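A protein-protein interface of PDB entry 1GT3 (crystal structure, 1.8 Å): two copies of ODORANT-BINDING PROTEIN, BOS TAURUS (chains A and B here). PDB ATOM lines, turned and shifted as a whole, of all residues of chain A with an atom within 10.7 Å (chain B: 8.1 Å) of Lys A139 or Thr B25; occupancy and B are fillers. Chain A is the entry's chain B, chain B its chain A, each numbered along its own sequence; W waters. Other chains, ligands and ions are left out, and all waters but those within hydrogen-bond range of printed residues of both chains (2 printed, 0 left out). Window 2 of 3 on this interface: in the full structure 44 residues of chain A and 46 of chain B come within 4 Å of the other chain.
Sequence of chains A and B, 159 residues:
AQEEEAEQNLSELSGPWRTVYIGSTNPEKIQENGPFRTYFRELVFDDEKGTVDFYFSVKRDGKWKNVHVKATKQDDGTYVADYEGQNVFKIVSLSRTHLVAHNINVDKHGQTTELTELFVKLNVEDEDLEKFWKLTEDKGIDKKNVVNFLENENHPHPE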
ATOM      1  N   LYS A 131       1.780  -5.344  -8.745  1.00  0.00           N
ATOM      2  CA  LYS A 131       0.734  -5.118  -9.736  1.00  0.00           C
ATOM      3  C   LYS A 131       1.267  -4.203 -10.820  1.00  0.00           C
ATOM      4  O   LYS A 131       1.026  -4.427 -12.005  1.00  0.00           O
ATOM      5  CB  LYS A 131      -0.497  -4.479  -9.097  1.00  0.00           C
ATOM      6  CG  LYS A 131      -1.252  -5.396  -8.150  1.00  0.00           C
ATOM      7  CD  LYS A 131      -2.329  -4.808  -7.246  1.00  0.00           C
ATOM      8  CE  LYS A 131      -3.079  -5.720  -6.300  1.00  0.00           C
ATOM      9  NZ  LYS A 131      -3.841  -4.943  -5.287  1.00  0.00           N
ATOM     10  N   PHE A 132       1.992  -3.165 -10.411  1.00  0.00           N
ATOM     11  CA  PHE A 132       2.564  -2.229 -11.369  1.00  0.00           C
ATOM     12  C   PHE A 132       3.569  -2.911 -12.283  1.00  0.00           C
ATOM     13  O   PHE A 132       3.521  -2.733 -13.496  1.00  0.00           O
ATOM     14  CB  PHE A 132       3.271  -1.075 -10.656  1.00  0.00           C
ATOM     15  CG  PHE A 132       4.096  -0.231 -11.573  1.00  0.00           C
ATOM     16  CD1 PHE A 132       3.489   0.655 -12.463  1.00  0.00           C
ATOM     17  CD2 PHE A 132       5.483  -0.366 -11.597  1.00  0.00           C
ATOM     18  CE1 PHE A 132       4.257   1.393 -13.366  1.00  0.00           C
ATOM     19  CE2 PHE A 132       6.257   0.364 -12.495  1.00  0.00           C
ATOM     20  CZ  PHE A 132       5.644   1.246 -13.383  1.00  0.00           C
ATOM     21  N   TRP A 133       4.493  -3.678 -11.711  1.00  0.00           N
ATOM     22  CA  TRP A 133       5.491  -4.333 -12.543  1.00  0.00           C
ATOM     23  C   TRP A 133       4.900  -5.396 -13.465  1.00  0.00           C
ATOM     24  O   TRP A 133       5.387  -5.584 -14.575  1.00  0.00           O
ATOM     25  CB  TRP A 133       6.607  -4.935 -11.686  1.00  0.00           C
ATOM     26  CG  TRP A 133       7.521  -3.891 -11.115  1.00  0.00           C
ATOM     27  CD1 TRP A 133       7.647  -3.532  -9.804  1.00  0.00           C
ATOM     28  CD2 TRP A 133       8.423  -3.059 -11.852  1.00  0.00           C
ATOM     29  NE1 TRP A 133       8.575  -2.526  -9.677  1.00  0.00           N
ATOM     30  CE2 TRP A 133       9.069  -2.216 -10.917  1.00  0.00           C
ATOM     31  CE3 TRP A 133       8.753  -2.941 -13.208  1.00  0.00           C
ATOM     32  CZ2 TRP A 133      10.029  -1.266 -11.300  1.00  0.00           C
ATOM     33  CZ3 TRP A 133       9.707  -1.998 -13.590  1.00  0.00           C
ATOM     34  CH2 TRP A 133      10.332  -1.175 -12.634  1.00  0.00           C
ATOM     35  N   LYS A 134       3.859  -6.082 -13.012  1.00  0.00           N
ATOM     36  CA  LYS A 134       3.215  -7.104 -13.836  1.00  0.00           C
ATOM     37  C   LYS A 134       2.574  -6.443 -15.053  1.00  0.00           C
ATOM     38  O   LYS A 134       2.749  -6.893 -16.191  1.00  0.00           O
ATOM     39  CB  LYS A 134       2.153  -7.847 -13.017  1.00  0.00           C
ATOM     40  CG  LYS A 134       1.415  -8.980 -13.779  1.00  0.00           C
ATOM     41  CD  LYS A 134       2.172 -10.002 -14.595  1.00  0.00           C
ATOM     42  CE  LYS A 134       1.431 -11.122 -15.327  1.00  0.00           C
ATOM     43  NZ  LYS A 134       0.314 -10.634 -16.186  1.00  0.00           N
ATOM     44  N   LEU A 135       1.833  -5.366 -14.810  1.00  0.00           N
ATOM     45  CA  LEU A 135       1.174  -4.631 -15.885  1.00  0.00           C
ATOM     46  C   LEU A 135       2.210  -4.066 -16.845  1.00  0.00           C
ATOM     47  O   LEU A 135       2.002  -4.027 -18.060  1.00  0.00           O
ATOM     48  CB  LEU A 135       0.351  -3.476 -15.310  1.00  0.00           C
ATOM     49  CG  LEU A 135      -0.232  -2.471 -16.307  1.00  0.00           C
ATOM     50  CD1 LEU A 135      -1.281  -3.148 -17.182  1.00  0.00           C
ATOM     51  CD2 LEU A 135      -0.842  -1.306 -15.538  1.00  0.00           C
ATOM     52  N   THR A 136       3.329  -3.615 -16.288  1.00  0.00           N
ATOM     53  CA  THR A 136       4.386  -3.035 -17.095  1.00  0.00           C
ATOM     54  C   THR A 136       4.999  -4.088 -18.005  1.00  0.00           C
ATOM     55  O   THR A 136       5.293  -3.814 -19.169  1.00  0.00           O
ATOM     56  CB  THR A 136       5.471  -2.387 -16.193  1.00  0.00           C
ATOM     57  OG1 THR A 136       4.889  -1.290 -15.473  1.00  0.00           O
ATOM     58  CG2 THR A 136       6.642  -1.875 -17.028  1.00  0.00           C
ATOM     59  N   GLU A 137       5.179  -5.302 -17.499  1.00  0.00           N
ATOM     60  CA  GLU A 137       5.756  -6.325 -18.353  1.00  0.00           C
ATOM     61  C   GLU A 137       4.719  -6.850 -19.346  1.00  0.00           C
ATOM     62  O   GLU A 137       5.074  -7.277 -20.445  1.00  0.00           O
ATOM     63  CB  GLU A 137       6.387  -7.445 -17.517  1.00  0.00           C
ATOM     64  CG  GLU A 137       5.538  -8.036 -16.458  1.00  0.00           C
ATOM     65  CD  GLU A 137       6.374  -8.625 -15.334  1.00  0.00           C
ATOM     66  OE1 GLU A 137       5.828  -9.397 -14.521  1.00  0.00           O
ATOM     67  OE2 GLU A 137       7.580  -8.306 -15.258  1.00  0.00           O
ATOM     68  N   ASP A 138       3.438  -6.788 -18.972  1.00  0.00           N
ATOM     69  CA  ASP A 138       2.365  -7.223 -19.867  1.00  0.00           C
ATOM     70  C   ASP A 138       2.356  -6.340 -21.117  1.00  0.00           C
ATOM     71  O   ASP A 138       2.019  -6.795 -22.211  1.00  0.00           O
ATOM     72  CB  ASP A 138       0.984  -7.102 -19.196  1.00  0.00           C
ATOM     73  CG  ASP A 138       0.684  -8.244 -18.243  1.00  0.00           C
ATOM     74  OD1 ASP A 138       1.444  -9.229 -18.223  1.00  0.00           O
ATOM     75  OD2 ASP A 138      -0.329  -8.153 -17.517  1.00  0.00           O
ATOM     76  N   LYS A 139       2.722  -5.074 -20.949  1.00  0.00           N
ATOM     77  CA  LYS A 139       2.723  -4.140 -22.068  1.00  0.00           C
ATOM     78  C   LYS A 139       4.038  -4.079 -22.827  1.00  0.00           C
ATOM     79  O   LYS A 139       4.223  -3.218 -23.686  1.00  0.00           O
ATOM     80  CB  LYS A 139       2.336  -2.743 -21.579  1.00  0.00           C
ATOM     81  CG  LYS A 139       1.000  -2.722 -20.903  1.00  0.00           C
ATOM     82  CD  LYS A 139      -0.154  -3.370 -21.656  1.00  0.00           C
ATOM     83  CE  LYS A 139      -1.558  -3.433 -21.109  1.00  0.00           C
ATOM     84  NZ  LYS A 139      -2.466  -4.087 -22.099  1.00  0.00           N
ATOM     85  N   GLY A 140       4.948  -4.993 -22.513  1.00  0.00           N
ATOM     86  CA  GLY A 140       6.226  -5.020 -23.201  1.00  0.00           C
ATOM     87  C   GLY A 140       7.115  -3.816 -22.956  1.00  0.00           C
ATOM     88  O   GLY A 140       7.885  -3.421 -23.834  1.00  0.00           O
ATOM     89  N   ILE A 141       7.011  -3.226 -21.769  1.00  0.00           N
ATOM     90  CA  ILE A 141       7.829  -2.069 -21.427  1.00  0.00           C
ATOM     91  C   ILE A 141       9.093  -2.535 -20.717  1.00  0.00           C
ATOM     92  O   ILE A 141       9.031  -3.284 -19.744  1.00  0.00           O
ATOM     93  CB  ILE A 141       7.060  -1.081 -20.517  1.00  0.00           C
ATOM     94  CG1 ILE A 141       5.928  -0.426 -21.312  1.00  0.00           C
ATOM     95  CG2 ILE A 141       8.009  -0.022 -19.967  1.00  0.00           C
ATOM     96  CD1 ILE A 141       5.022   0.483 -20.486  1.00  0.00           C
ATOM     97  N   ASP A 142      10.239  -2.095 -21.224  1.00  0.00           N
ATOM     98  CA  ASP A 142      11.533  -2.456 -20.655  1.00  0.00           C
ATOM     99  C   ASP A 142      11.719  -1.733 -19.318  1.00  0.00           C
ATOM    100  O   ASP A 142      11.307  -0.588 -19.161  1.00  0.00           O
ATOM    101  CB  ASP A 142      12.652  -2.061 -21.629  1.00  0.00           C
ATOM    102  CG  ASP A 142      13.988  -2.693 -21.278  1.00  0.00           C
ATOM    103  OD1 ASP A 142      14.475  -2.484 -20.146  1.00  0.00           O
ATOM    104  OD2 ASP A 142      14.555  -3.401 -22.138  1.00  0.00           O
ATOM    105  N   LYS A 143      12.337  -2.411 -18.357  1.00  0.00           N
ATOM    106  CA  LYS A 143      12.575  -1.830 -17.037  1.00  0.00           C
ATOM    107  C   LYS A 143      13.381  -0.541 -17.064  1.00  0.00           C
ATOM    108  O   LYS A 143      13.258   0.290 -16.165  1.00  0.00           O
ATOM    109  CB  LYS A 143      13.276  -2.840 -16.138  1.00  0.00           C
ATOM    110  CG  LYS A 143      12.334  -3.782 -15.452  1.00  0.00           C
ATOM    111  CD  LYS A 143      12.868  -4.955 -14.672  1.00  0.00           C
ATOM    112  CE  LYS A 143      11.891  -5.863 -13.995  1.00  0.00           C
ATOM    113  NZ  LYS A 143      11.146  -5.114 -12.942  1.00  0.00           N
ATOM    114  N   LYS A 144      14.208  -0.371 -18.087  1.00  0.00           N
ATOM    115  CA  LYS A 144      15.011   0.839 -18.193  1.00  0.00           C
ATOM    116  C   LYS A 144      14.220   2.010 -18.714  1.00  0.00           C
ATOM    117  O   LYS A 144      14.706   3.138 -18.742  1.00  0.00           O
ATOM    118  CB  LYS A 144      16.229   0.583 -19.076  1.00  0.00           C
ATOM    119  CG  LYS A 144      17.103  -0.379 -18.432  1.00  0.00           C
ATOM    120  CD  LYS A 144      17.176  -0.046 -16.962  1.00  0.00           C
ATOM    121  CE  LYS A 144      17.915  -0.800 -16.084  1.00  0.00           C
ATOM    122  NZ  LYS A 144      17.908  -0.288 -14.693  1.00  0.00           N
ATOM    123  N   ASN A 145      12.990   1.730 -19.121  1.00  0.00           N
ATOM    124  CA  ASN A 145      12.105   2.756 -19.639  1.00  0.00           C
ATOM    125  C   ASN A 145      11.059   3.102 -18.582  1.00  0.00           C
ATOM    126  O   ASN A 145       9.916   3.436 -18.892  1.00  0.00           O
ATOM    127  CB  ASN A 145      11.453   2.259 -20.930  1.00  0.00           C
ATOM    128  CG  ASN A 145      12.435   2.227 -22.089  1.00  0.00           C
ATOM    129  OD1 ASN A 145      12.192   1.584 -23.109  1.00  0.00           O
ATOM    130  ND2 ASN A 145      13.550   2.933 -21.938  1.00  0.00           N
ATOM    131  N   VAL A 146      11.479   3.010 -17.326  1.00  0.00           N
ATOM    132  CA  VAL A 146      10.630   3.322 -16.188  1.00  0.00           C
ATOM    133  C   VAL A 146      11.351   4.337 -15.307  1.00  0.00           C
ATOM    134  O   VAL A 146      12.524   4.162 -14.972  1.00  0.00           O
ATOM    135  CB  VAL A 146      10.319   2.060 -15.355  1.00  0.00           C
ATOM    136  CG1 VAL A 146       9.465   2.431 -14.146  1.00  0.00           C
ATOM    137  CG2 VAL A 146       9.606   1.027 -16.230  1.00  0.00           C
ATOM    138  N   VAL A 147      10.646   5.399 -14.942  1.00  0.00           N
ATOM    139  CA  VAL A 147      11.203   6.452 -14.106  1.00  0.00           C
ATOM    140  C   VAL A 147      10.635   6.398 -12.689  1.00  0.00           C
ATOM    141  O   VAL A 147       9.441   6.173 -12.493  1.00  0.00           O
ATOM    142  CB  VAL A 147      10.898   7.846 -14.699  1.00  0.00           C
ATOM    143  CG1 VAL A 147      11.303   8.941 -13.713  1.00  0.00           C
ATOM    144  CG2 VAL A 147      11.636   8.021 -16.013  1.00  0.00           C
ATOM    145  N   ILE B  22       6.343   5.672 -13.557  1.00  0.00           N
ATOM    146  CA  ILE B  22       5.684   5.777 -14.854  1.00  0.00           C
ATOM    147  C   ILE B  22       6.608   5.049 -15.830  1.00  0.00           C
ATOM    148  O   ILE B  22       7.814   5.273 -15.830  1.00  0.00           O
ATOM    149  CB  ILE B  22       5.482   7.239 -15.347  1.00  0.00           C
ATOM    150  CG1 ILE B  22       4.476   7.968 -14.452  1.00  0.00           C
ATOM    151  CG2 ILE B  22       4.925   7.228 -16.775  1.00  0.00           C
ATOM    152  CD1 ILE B  22       4.198   9.396 -14.891  1.00  0.00           C
ATOM    153  N   GLY B  23       6.039   4.155 -16.629  1.00  0.00           N
ATOM    154  CA  GLY B  23       6.818   3.426 -17.615  1.00  0.00           C
ATOM    155  C   GLY B  23       6.250   3.773 -18.981  1.00  0.00           C
ATOM    156  O   GLY B  23       5.085   4.143 -19.081  1.00  0.00           O
ATOM    157  N   SER B  24       7.051   3.651 -20.033  1.00  0.00           N
ATOM    158  CA  SER B  24       6.571   3.993 -21.369  1.00  0.00           C
ATOM    159  C   SER B  24       7.190   3.137 -22.464  1.00  0.00           C
ATOM    160  O   SER B  24       8.362   2.771 -22.386  1.00  0.00           O
ATOM    161  CB  SER B  24       6.873   5.463 -21.666  1.00  0.00           C
ATOM    162  OG  SER B  24       6.439   5.812 -22.967  1.00  0.00           O
ATOM    163  N   THR B  25       6.399   2.816 -23.488  1.00  0.00           N
ATOM    164  CA  THR B  25       6.908   2.016 -24.600  1.00  0.00           C
ATOM    165  C   THR B  25       7.837   2.886 -25.450  1.00  0.00           C
ATOM    166  O   THR B  25       8.625   2.377 -26.251  1.00  0.00           O
ATOM    167  CB  THR B  25       5.754   1.444 -25.482  1.00  0.00           C
ATOM    168  OG1 THR B  25       4.839   2.487 -25.834  1.00  0.00           O
ATOM    169  CG2 THR B  25       5.005   0.349 -24.734  1.00  0.00           C
ATOM    170  N   ASN B  26       7.737   4.198 -25.256  1.00  0.00           N
ATOM    171  CA  ASN B  26       8.573   5.179 -25.954  1.00  0.00           C
ATOM    172  C   ASN B  26       9.237   6.026 -24.869  1.00  0.00           C
ATOM    173  O   ASN B  26       8.618   6.939 -24.321  1.00  0.00           O
ATOM    174  CB  ASN B  26       7.727   6.092 -26.846  1.00  0.00           C
ATOM    175  CG  ASN B  26       8.580   7.039 -27.680  1.00  0.00           C
ATOM    176  OD1 ASN B  26       9.637   7.495 -27.235  1.00  0.00           O
ATOM    177  ND2 ASN B  26       8.118   7.348 -28.891  1.00  0.00           N
ATOM    178  N   PRO B  27      10.515   5.747 -24.558  1.00  0.00           N
ATOM    179  CA  PRO B  27      11.263   6.477 -23.528  1.00  0.00           C
ATOM    180  C   PRO B  27      11.307   7.998 -23.664  1.00  0.00           C
ATOM    181  O   PRO B  27      11.377   8.708 -22.665  1.00  0.00           O
ATOM    182  CB  PRO B  27      12.649   5.836 -23.591  1.00  0.00           C
ATOM    183  CG  PRO B  27      12.768   5.444 -25.034  1.00  0.00           C
ATOM    184  CD  PRO B  27      11.409   4.850 -25.313  1.00  0.00           C
ATOM    185  N   GLU B  28      11.263   8.497 -24.894  1.00  0.00           N
ATOM    186  CA  GLU B  28      11.306   9.937 -25.138  1.00  0.00           C
ATOM    187  C   GLU B  28      10.175  10.687 -24.434  1.00  0.00           C
ATOM    188  O   GLU B  28      10.360  11.816 -23.975  1.00  0.00           O
ATOM    189  CB  GLU B  28      11.230  10.212 -26.643  1.00  0.00           C
ATOM    190  CG  GLU B  28      12.444   9.728 -27.441  1.00  0.00           C
ATOM    191  CD  GLU B  28      12.215   9.792 -28.941  1.00  0.00           C
ATOM    192  OE1 GLU B  28      11.426   8.973 -29.462  1.00  0.00           O
ATOM    193  OE2 GLU B  28      12.816  10.666 -29.599  1.00  0.00           O
ATOM    194  N   LYS B  29       9.007  10.057 -24.356  1.00  0.00           N
ATOM    195  CA  LYS B  29       7.839  10.671 -23.724  1.00  0.00           C
ATOM    196  C   LYS B  29       7.996  10.933 -22.225  1.00  0.00           C
ATOM    197  O   LYS B  29       7.341  11.820 -21.678  1.00  0.00           O
ATOM    198  CB  LYS B  29       6.601   9.802 -23.958  1.00  0.00           C
ATOM    199  CG  LYS B  29       6.224   9.651 -25.423  1.00  0.00           C
ATOM    200  CD  LYS B  29       5.822  10.877 -26.237  1.00  0.00           C
ATOM    201  CE  LYS B  29       5.446  10.725 -27.711  1.00  0.00           C
ATOM    202  NZ  LYS B  29       4.856  11.973 -28.249  1.00  0.00           N
ATOM    203  N   ILE B  30       8.859  10.170 -21.558  1.00  0.00           N
ATOM    204  CA  ILE B  30       9.040  10.361 -20.120  1.00  0.00           C
ATOM    205  C   ILE B  30      10.436  10.821 -19.701  1.00  0.00           C
ATOM    206  O   ILE B  30      10.697  11.034 -18.513  1.00  0.00           O
ATOM    207  CB  ILE B  30       8.658   9.084 -19.335  1.00  0.00           C
ATOM    208  CG1 ILE B  30       9.516   7.901 -19.780  1.00  0.00           C
ATOM    209  CG2 ILE B  30       7.183   8.776 -19.556  1.00  0.00           C
ATOM    210  CD1 ILE B  30       9.277   6.638 -18.980  1.00  0.00           C
ATOM    211  N   VAL B  92      -6.494   0.013 -13.707  1.00  0.00           N
ATOM    212  CA  VAL B  92      -6.332  -1.425 -13.557  1.00  0.00           C
ATOM    213  C   VAL B  92      -6.528  -1.880 -12.110  1.00  0.00           C
ATOM    214  O   VAL B  92      -7.202  -2.876 -11.855  1.00  0.00           O
ATOM    215  CB  VAL B  92      -4.934  -1.861 -14.058  1.00  0.00           C
ATOM    216  CG1 VAL B  92      -4.772  -3.366 -13.933  1.00  0.00           C
ATOM    217  CG2 VAL B  92      -4.748  -1.427 -15.507  1.00  0.00           C
ATOM    218  N   ALA B 101      -2.563   2.451 -13.235  1.00  0.00           N
ATOM    219  CA  ALA B 101      -3.286   2.720 -14.468  1.00  0.00           C
ATOM    220  C   ALA B 101      -2.479   2.450 -15.726  1.00  0.00           C
ATOM    221  O   ALA B 101      -1.249   2.369 -15.692  1.00  0.00           O
ATOM    222  CB  ALA B 101      -3.774   4.161 -14.470  1.00  0.00           C
ATOM    223  N   HIS B 102      -3.205   2.315 -16.833  1.00  0.00           N
ATOM    224  CA  HIS B 102      -2.640   2.060 -18.150  1.00  0.00           C
ATOM    225  C   HIS B 102      -3.183   3.162 -19.060  1.00  0.00           C
ATOM    226  O   HIS B 102      -4.387   3.419 -19.069  1.00  0.00           O
ATOM    227  CB  HIS B 102      -3.112   0.689 -18.647  1.00  0.00           C
ATOM    228  CG  HIS B 102      -2.762   0.398 -20.073  1.00  0.00           C
ATOM    229  ND1 HIS B 102      -3.467  -0.507 -20.838  1.00  0.00           N
ATOM    230  CD2 HIS B 102      -1.775   0.875 -20.870  1.00  0.00           C
ATOM    231  CE1 HIS B 102      -2.932  -0.574 -22.043  1.00  0.00           C
ATOM    232  NE2 HIS B 102      -1.903   0.254 -22.089  1.00  0.00           N
ATOM    233  N   ASN B 103      -2.305   3.819 -19.813  1.00  0.00           N
ATOM    234  CA  ASN B 103      -2.746   4.882 -20.712  1.00  0.00           C
ATOM    235  C   ASN B 103      -2.221   4.700 -22.134  1.00  0.00           C
ATOM    236  O   ASN B 103      -1.064   4.336 -22.344  1.00  0.00           O
ATOM    237  CB  ASN B 103      -2.296   6.249 -20.185  1.00  0.00           C
ATOM    238  CG  ASN B 103      -2.800   7.407 -21.041  1.00  0.00           C
ATOM    239  OD1 ASN B 103      -2.023   8.095 -21.709  1.00  0.00           O
ATOM    240  ND2 ASN B 103      -4.106   7.624 -21.019  1.00  0.00           N
ATOM    241  N   ILE B 104      -3.093   4.936 -23.110  1.00  0.00           N
ATOM    242  CA  ILE B 104      -2.706   4.846 -24.511  1.00  0.00           C
ATOM    243  C   ILE B 104      -2.794   6.259 -25.079  1.00  0.00           C
ATOM    244  O   ILE B 104      -3.853   6.887 -25.046  1.00  0.00           O
ATOM    245  CB  ILE B 104      -3.637   3.912 -25.315  1.00  0.00           C
ATOM    246  CG1 ILE B 104      -3.579   2.497 -24.727  1.00  0.00           C
ATOM    247  CG2 ILE B 104      -3.205   3.885 -26.783  1.00  0.00           C
ATOM    248  CD1 ILE B 104      -4.566   1.528 -25.341  1.00  0.00           C
ATOM    249  N   ASN B 105      -1.671   6.757 -25.574  1.00  0.00           N
ATOM    250  CA  ASN B 105      -1.615   8.093 -26.141  1.00  0.00           C
ATOM    251  C   ASN B 105      -1.262   8.031 -27.619  1.00  0.00           C
ATOM    252  O   ASN B 105      -0.441   7.219 -28.041  1.00  0.00           O
ATOM    253  CB  ASN B 105      -0.579   8.937 -25.386  1.00  0.00           C
ATOM    254  CG  ASN B 105      -0.342  10.294 -26.029  1.00  0.00           C
ATOM    255  OD1 ASN B 105       0.558  10.454 -26.855  1.00  0.00           O
ATOM    256  ND2 ASN B 105      -1.154  11.276 -25.658  1.00  0.00           N
ATOM    257  N   THR B 112       1.703   5.997 -31.511  1.00  0.00           N
ATOM    258  CA  THR B 112       1.055   5.387 -30.356  1.00  0.00           C
ATOM    259  C   THR B 112       2.066   5.048 -29.254  1.00  0.00           C
ATOM    260  O   THR B 112       3.094   4.432 -29.510  1.00  0.00           O
ATOM    261  CB  THR B 112       0.316   4.097 -30.768  1.00  0.00           C
ATOM    262  OG1 THR B 112      -0.658   4.404 -31.772  1.00  0.00           O
ATOM    263  CG2 THR B 112      -0.384   3.469 -29.571  1.00  0.00           C
ATOM    264  N   THR B 113       1.762   5.463 -28.026  1.00  0.00           N
ATOM    265  CA  THR B 113       2.628   5.194 -26.882  1.00  0.00           C
ATOM    266  C   THR B 113       1.784   4.636 -25.745  1.00  0.00           C
ATOM    267  O   THR B 113       0.743   5.199 -25.416  1.00  0.00           O
ATOM    268  CB  THR B 113       3.303   6.481 -26.370  1.00  0.00           C
ATOM    269  OG1 THR B 113       4.073   7.077 -27.421  1.00  0.00           O
ATOM    270  CG2 THR B 113       4.227   6.167 -25.190  1.00  0.00           C
ATOM    271  N   GLU B 114       2.209   3.517 -25.161  1.00  0.00           N
ATOM    272  CA  GLU B 114       1.475   2.956 -24.035  1.00  0.00           C
ATOM    273  C   GLU B 114       2.275   3.245 -22.767  1.00  0.00           C
ATOM    274  O   GLU B 114       3.496   3.092 -22.742  1.00  0.00           O
ATOM    275  CB  GLU B 114       1.264   1.449 -24.207  1.00  0.00           C
ATOM    276  CG  GLU B 114       0.511   1.092 -25.518  1.00  0.00           C
ATOM    277  CD  GLU B 114      -0.222  -0.227 -25.443  1.00  0.00           C
ATOM    278  OE1 GLU B 114      -0.369  -0.887 -26.494  1.00  0.00           O
ATOM    279  OE2 GLU B 114      -0.667  -0.603 -24.339  1.00  0.00           O
ATOM    280  N   LEU B 115       1.583   3.691 -21.726  1.00  0.00           N
ATOM    281  CA  LEU B 115       2.244   4.019 -20.472  1.00  0.00           C
ATOM    282  C   LEU B 115       1.556   3.318 -19.321  1.00  0.00           C
ATOM    283  O   LEU B 115       0.356   3.046 -19.380  1.00  0.00           O
ATOM    284  CB  LEU B 115       2.213   5.528 -20.227  1.00  0.00           C
ATOM    285  CG  LEU B 115       2.803   6.441 -21.308  1.00  0.00           C
ATOM    286  CD1 LEU B 115       1.661   7.072 -22.109  1.00  0.00           C
ATOM    287  CD2 LEU B 115       3.653   7.530 -20.665  1.00  0.00           C
ATOM    288  N   THR B 116       2.332   3.010 -18.287  1.00  0.00           N
ATOM    289  CA  THR B 116       1.812   2.360 -17.097  1.00  0.00           C
ATOM    290  C   THR B 116       2.223   3.277 -15.959  1.00  0.00           C
ATOM    291  O   THR B 116       3.222   3.991 -16.062  1.00  0.00           O
ATOM    292  CB  THR B 116       2.439   0.962 -16.858  1.00  0.00           C
ATOM    293  OG1 THR B 116       3.866   1.079 -16.789  1.00  0.00           O
ATOM    294  CG2 THR B 116       2.055  -0.002 -17.978  1.00  0.00           C
HETATM  295  O   HOH W   1      -2.486  -2.706 -24.428  1.00  0.00           O
HETATM  296  O   HOH W   2       9.870   0.592 -23.197  1.00  0.00           O
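The backbone carbonyl oxygen (O) of Ile B22 sits at hydrogen-bond distance from the backbone NH (N) of Val A147, 3.0 Å away. O of Asn A145 is in hydrogen-bond range of N of Ser B24. OG1 of Thr B116 sits at hydrogen-bond distance from OG1 of Thr A136 (2.9 Å).
The backbone carbonyl oxygen (O) of Thr B116 is in hydrogen-bond range of the backbone NH (N) of Gly B23 (2.9 Å). The backbone carbonyl oxygen (O) of Asn B26 lies within hydrogen-bond range of the side-chain hydroxyl (OG) of Ser B24 (2.8 Å). The side-chain hydroxyl (OG1) of Thr B25 sits at hydrogen-bond distance from the backbone NH (N) of Glu B114 (2.9 Å). A ring nitrogen (NE2) of His B102 lies within hydrogen-bond range of the side-chain carboxylate (OE2) of Glu B114 (2.7 Å). The backbone carbonyl oxygen of Phe A132 lies within hydrogen-bond range of the side-chain hydroxyl of Thr A136. The backbone NH (N) of Ile A141 sits at hydrogen-bond distance from the backbone carbonyl oxygen (O) of Thr A136 (3.2 Å).
OG1 of Thr B116 touches CE1 of Phe A132, 3.5 Å away. Ala B101 touches Leu A135. Lys A139 touches Thr B25 (O to CG2, 3.8 Å). His B102 touches Lys A139. Lys A139 touches Glu B114 (CD to OE2, 3.9 Å). Ser B24 touches Ile A141 (O to CG2, 3.7 Å). Ile A141 touches Thr B25. CD1 of Ile A141 touches CG2 of Thr B116, at 3.9 Å. Gly B23 touches Asn A145. Gly B23 touches Val A146.
Of chain B, only Thr B25, His B102 and Glu B114 come within 4 Å of Lys A139. Gly A140 touches none of the printed residues of chain B. Of the printed residues of chain A, Gly B23 touches Ile A141 (3.8 Å), Asn A145 (3.4 Å) and Val A146 (3.9 Å). Of chain A, only Ile A141 and Asn A145 come within 4 Å of Ser B24. Thr B25 touches just these residues of chain A: Lys A139 and Ile A141. No residue of chain A comes within 4 Å of Asn B26. Printed residues of chain A within 4 Å of Ile B30: Asn A145 (3.3 Å). Asn B103 touches none of the printed residues of chain A. Of chain A, only Lys A139 and Ile A141 come within 4 Å of Glu B114. No residue of chain A comes within 4 Å of Leu B115. The nearest residue of chain B that does not touch Lys A139 is Thr B116 (4.1 Å). The nearest printed residue of chain A that does not touch Thr B25 is Asn A145 (4.8 Å). The nearest printed residue of chain B that does not touch Val A146 is Ile B30 (4.5 Å).
Of the 17 printed residues of chain A, 8 touch a printed residue of chain B. Hydrophobic or aromatic side chains of chain A that line the printed part of chain B: Phe A132, Leu A135, Ile A141 and Val A146. Along chain A the printed residues that touch a printed residue of chain B span positions 132 to 147. Among the printed residues, no Asp or Glu carboxylate lies within 4 Å of a Lys or Arg side-chain nitrogen of the other chain.
No position is printed for both chains.
Water W2 lies within hydrogen-bond range of OD1 of Asn A145, O of Ser B24 and N of Asp A142. Water W1 bridges NZ of Lys A139 (2.7 Å) and OE2 of Glu B114 (2.8 Å).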
